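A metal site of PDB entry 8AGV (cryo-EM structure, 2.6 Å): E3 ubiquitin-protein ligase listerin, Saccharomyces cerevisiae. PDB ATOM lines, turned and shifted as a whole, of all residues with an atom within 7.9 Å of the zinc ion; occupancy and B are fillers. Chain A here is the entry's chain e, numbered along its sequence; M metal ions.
The side-chain hydroxyl (OG) of Ser 1513 sits close to the side-chain sulfur (SG) of Cys 1511 (3.0 Å).
A ring nitrogen (NE2) of His 1535 sits close to the backbone carbonyl oxygen of Lys 1521, 3.4 Å away.
The backbone carbonyl oxygen (O) of Ser 1513 lies close to a ring nitrogen (NE2) of His 1535 (3.3 Å).
O of Ser 1513 sits at hydrogen-bond distance from N of Cys 1508, at 3.0 Å.
The side-chain sulfur (SG) of Cys 1508 lies close to the backbone NH (N) of Ile 1510, 3.5 Å away.
The backbone carbonyl oxygen (O) of Ile 1514 is in hydrogen-bond range of a ring nitrogen (NE2) of His 1535, 3.1 Å away.
SG of Cys 1538 sits close to NE2 of His 1516 (3.6 Å).
NE2 of His 1535 is in hydrogen-bond range of N of His 1516 (3.3 Å).
Of the 20 residues printed, 4 come within 4 Å of the zinc ion.
ND1 of His 1535 binds the zinc ion (2.1 Å).
The side-chain sulfur (SG) of Cys 1508 binds the zinc ion (2.3 Å).
The side-chain sulfur (SG) of Cys 1511 is bound to the zinc ion, at 2.3 Å.
SG of Cys 1538 is bound to the zinc ion (2.3 Å).
The zinc ion has four donor atoms within binding distance.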
ATOM      1  N   GLU A1507      13.847  16.684  33.253  1.00  0.00           N
ATOM      2  CA  GLU A1507      15.230  17.110  33.178  1.00  0.00           C
ATOM      3  C   GLU A1507      15.930  16.477  31.992  1.00  0.00           C
ATOM      4  O   GLU A1507      15.607  15.358  31.601  1.00  0.00           O
ATOM      5  CB  GLU A1507      15.964  16.754  34.464  1.00  0.00           C
ATOM      6  CG  GLU A1507      15.384  17.396  35.707  1.00  0.00           C
ATOM      7  CD  GLU A1507      16.140  17.036  36.958  1.00  0.00           C
ATOM      8  OE1 GLU A1507      16.746  15.949  36.981  1.00  0.00           O
ATOM      9  OE2 GLU A1507      16.117  17.824  37.927  1.00  0.00           O
ATOM     10  N   CYS A1508      16.902  17.182  31.414  1.00  0.00           N
ATOM     11  CA  CYS A1508      17.658  16.611  30.316  1.00  0.00           C
ATOM     12  C   CYS A1508      18.433  15.404  30.788  1.00  0.00           C
ATOM     13  O   CYS A1508      19.022  15.442  31.854  1.00  0.00           O
ATOM     14  CB  CYS A1508      18.602  17.662  29.765  1.00  0.00           C
ATOM     15  SG  CYS A1508      20.041  17.058  28.845  1.00  0.00           S
ATOM     16  N   ALA A1509      18.425  14.324  30.022  1.00  0.00           N
ATOM     17  CA  ALA A1509      19.086  13.101  30.460  1.00  0.00           C
ATOM     18  C   ALA A1509      20.594  13.220  30.631  1.00  0.00           C
ATOM     19  O   ALA A1509      21.154  12.715  31.601  1.00  0.00           O
ATOM     20  CB  ALA A1509      18.755  11.963  29.516  1.00  0.00           C
ATOM     21  N   ILE A1510      21.251  13.892  29.689  1.00  0.00           N
ATOM     22  CA  ILE A1510      22.708  14.015  29.760  1.00  0.00           C
ATOM     23  C   ILE A1510      23.191  14.800  30.980  1.00  0.00           C
ATOM     24  O   ILE A1510      24.130  14.368  31.655  1.00  0.00           O
ATOM     25  CB  ILE A1510      23.275  14.639  28.472  1.00  0.00           C
ATOM     26  CG1 ILE A1510      22.751  13.879  27.248  1.00  0.00           C
ATOM     27  CG2 ILE A1510      24.789  14.647  28.477  1.00  0.00           C
ATOM     28  CD1 ILE A1510      23.349  14.341  25.948  1.00  0.00           C
ATOM     29  N   CYS A1511      22.549  15.925  31.283  1.00  0.00           N
ATOM     30  CA  CYS A1511      23.003  16.749  32.392  1.00  0.00           C
ATOM     31  C   CYS A1511      22.118  16.764  33.633  1.00  0.00           C
ATOM     32  O   CYS A1511      22.439  17.440  34.611  1.00  0.00           O
ATOM     33  CB  CYS A1511      23.264  18.180  31.920  1.00  0.00           C
ATOM     34  SG  CYS A1511      21.805  19.057  31.337  1.00  0.00           S
ATOM     35  N   TYR A1512      20.994  16.049  33.600  1.00  0.00           N
ATOM     36  CA  TYR A1512      20.088  15.965  34.758  1.00  0.00           C
ATOM     37  C   TYR A1512      19.623  17.329  35.270  1.00  0.00           C
ATOM     38  O   TYR A1512      19.496  17.521  36.477  1.00  0.00           O
ATOM     39  CB  TYR A1512      20.706  15.118  35.876  1.00  0.00           C
ATOM     40  CG  TYR A1512      19.686  14.289  36.637  1.00  0.00           C
ATOM     41  CD1 TYR A1512      18.879  13.380  35.977  1.00  0.00           C
ATOM     42  CD2 TYR A1512      19.552  14.425  38.017  1.00  0.00           C
ATOM     43  CE1 TYR A1512      17.960  12.617  36.668  1.00  0.00           C
ATOM     44  CE2 TYR A1512      18.625  13.673  38.710  1.00  0.00           C
ATOM     45  CZ  TYR A1512      17.836  12.770  38.034  1.00  0.00           C
ATOM     46  OH  TYR A1512      16.915  12.015  38.721  1.00  0.00           O
ATOM     47  N   SER A1513      19.368  18.266  34.362  1.00  0.00           N
ATOM     48  CA  SER A1513      18.857  19.569  34.766  1.00  0.00           C
ATOM     49  C   SER A1513      17.804  20.034  33.785  1.00  0.00           C
ATOM     50  O   SER A1513      17.925  19.799  32.591  1.00  0.00           O
ATOM     51  CB  SER A1513      19.992  20.581  34.812  1.00  0.00           C
ATOM     52  OG  SER A1513      20.624  20.709  33.554  1.00  0.00           O
ATOM     53  N   ILE A1514      16.750  20.674  34.279  1.00  0.00           N
ATOM     54  CA  ILE A1514      15.737  21.208  33.383  1.00  0.00           C
ATOM     55  C   ILE A1514      16.292  22.340  32.520  1.00  0.00           C
ATOM     56  O   ILE A1514      15.982  22.450  31.346  1.00  0.00           O
ATOM     57  CB  ILE A1514      14.483  21.671  34.134  1.00  0.00           C
ATOM     58  CG1 ILE A1514      14.247  20.803  35.371  1.00  0.00           C
ATOM     59  CG2 ILE A1514      13.274  21.609  33.219  1.00  0.00           C
ATOM     60  CD1 ILE A1514      12.929  21.072  36.059  1.00  0.00           C
ATOM     61  N   LEU A1515      17.127  23.184  33.109  1.00  0.00           N
ATOM     62  CA  LEU A1515      17.664  24.319  32.368  1.00  0.00           C
ATOM     63  C   LEU A1515      19.137  24.139  32.076  1.00  0.00           C
ATOM     64  O   LEU A1515      19.932  23.843  32.970  1.00  0.00           O
ATOM     65  CB  LEU A1515      17.439  25.623  33.153  1.00  0.00           C
ATOM     66  CG  LEU A1515      15.983  26.087  33.274  1.00  0.00           C
ATOM     67  CD1 LEU A1515      15.877  27.257  34.235  1.00  0.00           C
ATOM     68  CD2 LEU A1515      15.429  26.453  31.915  1.00  0.00           C
ATOM     69  N   HIS A1516      19.521  24.326  30.818  1.00  0.00           N
ATOM     70  CA  HIS A1516      20.925  24.205  30.440  1.00  0.00           C
ATOM     71  C   HIS A1516      21.661  25.298  31.180  1.00  0.00           C
ATOM     72  O   HIS A1516      21.201  26.429  31.219  1.00  0.00           O
ATOM     73  CB  HIS A1516      21.081  24.403  28.941  1.00  0.00           C
ATOM     74  CG  HIS A1516      22.390  23.905  28.391  1.00  0.00           C
ATOM     75  ND1 HIS A1516      23.519  24.701  28.322  1.00  0.00           N
ATOM     76  CD2 HIS A1516      22.748  22.710  27.878  1.00  0.00           C
ATOM     77  CE1 HIS A1516      24.506  24.009  27.795  1.00  0.00           C
ATOM     78  NE2 HIS A1516      24.067  22.789  27.518  1.00  0.00           N
ATOM     79  N   ALA A1517      22.786  24.975  31.796  1.00  0.00           N
ATOM     80  CA  ALA A1517      23.457  25.994  32.597  1.00  0.00           C
ATOM     81  C   ALA A1517      23.930  27.161  31.745  1.00  0.00           C
ATOM     82  O   ALA A1517      23.718  28.318  32.109  1.00  0.00           O
ATOM     83  CB  ALA A1517      24.618  25.384  33.361  1.00  0.00           C
ATOM     84  N   LYS A1521      17.975  27.093  29.008  1.00  0.00           N
ATOM     85  CA  LYS A1521      16.859  26.645  28.182  1.00  0.00           C
ATOM     86  C   LYS A1521      16.300  25.276  28.551  1.00  0.00           C
ATOM     87  O   LYS A1521      17.036  24.409  29.030  1.00  0.00           O
ATOM     88  CB  LYS A1521      17.269  26.654  26.706  1.00  0.00           C
ATOM     89  CG  LYS A1521      16.092  26.649  25.736  1.00  0.00           C
ATOM     90  CD  LYS A1521      16.534  26.228  24.345  1.00  0.00           C
ATOM     91  CE  LYS A1521      15.332  26.084  23.416  1.00  0.00           C
ATOM     92  NZ  LYS A1521      15.720  25.583  22.072  1.00  0.00           N
ATOM     93  N   PRO A1523      14.694  21.459  27.966  1.00  0.00           N
ATOM     94  CA  PRO A1523      15.231  20.486  27.018  1.00  0.00           C
ATOM     95  C   PRO A1523      14.253  20.198  25.901  1.00  0.00           C
ATOM     96  O   PRO A1523      13.394  19.333  26.037  1.00  0.00           O
ATOM     97  CB  PRO A1523      15.405  19.223  27.879  1.00  0.00           C
ATOM     98  CG  PRO A1523      15.230  19.658  29.296  1.00  0.00           C
ATOM     99  CD  PRO A1523      14.321  20.837  29.237  1.00  0.00           C
ATOM    100  N   LYS A1533      14.283  13.603  27.567  1.00  0.00           N
ATOM    101  CA  LYS A1533      14.448  14.896  26.910  1.00  0.00           C
ATOM    102  C   LYS A1533      15.883  15.362  27.001  1.00  0.00           C
ATOM    103  O   LYS A1533      16.476  15.323  28.079  1.00  0.00           O
ATOM    104  CB  LYS A1533      13.539  15.935  27.554  1.00  0.00           C
ATOM    105  CG  LYS A1533      12.059  15.654  27.425  1.00  0.00           C
ATOM    106  CD  LYS A1533      11.246  16.756  28.107  1.00  0.00           C
ATOM    107  CE  LYS A1533       9.759  16.469  28.044  1.00  0.00           C
ATOM    108  NZ  LYS A1533       8.979  17.412  28.897  1.00  0.00           N
ATOM    109  N   PHE A1534      16.450  15.809  25.891  1.00  0.00           N
ATOM    110  CA  PHE A1534      17.836  16.246  25.868  1.00  0.00           C
ATOM    111  C   PHE A1534      17.936  17.700  25.473  1.00  0.00           C
ATOM    112  O   PHE A1534      17.206  18.147  24.594  1.00  0.00           O
ATOM    113  CB  PHE A1534      18.647  15.429  24.860  1.00  0.00           C
ATOM    114  CG  PHE A1534      18.524  13.941  25.031  1.00  0.00           C
ATOM    115  CD1 PHE A1534      19.346  13.270  25.909  1.00  0.00           C
ATOM    116  CD2 PHE A1534      17.605  13.217  24.287  1.00  0.00           C
ATOM    117  CE1 PHE A1534      19.255  11.896  26.054  1.00  0.00           C
ATOM    118  CE2 PHE A1534      17.506  11.855  24.434  1.00  0.00           C
ATOM    119  CZ  PHE A1534      18.329  11.192  25.324  1.00  0.00           C
ATOM    120  N   HIS A1535      18.822  18.458  26.117  1.00  0.00           N
ATOM    121  CA  HIS A1535      19.032  19.822  25.674  1.00  0.00           C
ATOM    122  C   HIS A1535      19.656  19.689  24.307  1.00  0.00           C
ATOM    123  O   HIS A1535      20.427  18.762  24.064  1.00  0.00           O
ATOM    124  CB  HIS A1535      20.023  20.576  26.562  1.00  0.00           C
ATOM    125  CG  HIS A1535      19.544  20.811  27.951  1.00  0.00           C
ATOM    126  ND1 HIS A1535      20.229  20.359  29.058  1.00  0.00           N
ATOM    127  CD2 HIS A1535      18.460  21.476  28.422  1.00  0.00           C
ATOM    128  CE1 HIS A1535      19.576  20.732  30.153  1.00  0.00           C
ATOM    129  NE2 HIS A1535      18.502  21.406  29.795  1.00  0.00           N
ATOM    130  N   GLY A1536      19.341  20.607  23.413  1.00  0.00           N
ATOM    131  CA  GLY A1536      19.843  20.488  22.060  1.00  0.00           C
ATOM    132  C   GLY A1536      21.355  20.525  22.036  1.00  0.00           C
ATOM    133  O   GLY A1536      21.976  19.734  21.341  1.00  0.00           O
ATOM    134  N   ALA A1537      21.950  21.412  22.819  1.00  0.00           N
ATOM    135  CA  ALA A1537      23.396  21.536  22.839  1.00  0.00           C
ATOM    136  C   ALA A1537      24.079  20.272  23.355  1.00  0.00           C
ATOM    137  O   ALA A1537      25.063  19.816  22.774  1.00  0.00           O
ATOM    138  CB  ALA A1537      23.810  22.730  23.688  1.00  0.00           C
ATOM    139  N   CYS A1538      23.532  19.688  24.420  1.00  0.00           N
ATOM    140  CA  CYS A1538      24.107  18.465  24.965  1.00  0.00           C
ATOM    141  C   CYS A1538      24.006  17.339  23.947  1.00  0.00           C
ATOM    142  O   CYS A1538      24.962  16.593  23.752  1.00  0.00           O
ATOM    143  CB  CYS A1538      23.389  18.051  26.237  1.00  0.00           C
ATOM    144  SG  CYS A1538      23.437  19.219  27.608  1.00  0.00           S
ATOM    145  N   LEU A1539      22.865  17.234  23.290  1.00  0.00           N
ATOM    146  CA  LEU A1539      22.663  16.169  22.311  1.00  0.00           C
ATOM    147  C   LEU A1539      23.628  16.305  21.153  1.00  0.00           C
ATOM    148  O   LEU A1539      24.208  15.323  20.703  1.00  0.00           O
ATOM    149  CB  LEU A1539      21.231  16.192  21.792  1.00  0.00           C
ATOM    150  CG  LEU A1539      20.768  14.958  21.030  1.00  0.00           C
ATOM    151  CD1 LEU A1539      20.870  13.728  21.912  1.00  0.00           C
ATOM    152  CD2 LEU A1539      19.350  15.147  20.530  1.00  0.00           C
HETATM  153 ZN    ZN M   1      21.616  18.767  29.017  1.00  0.00          ZN
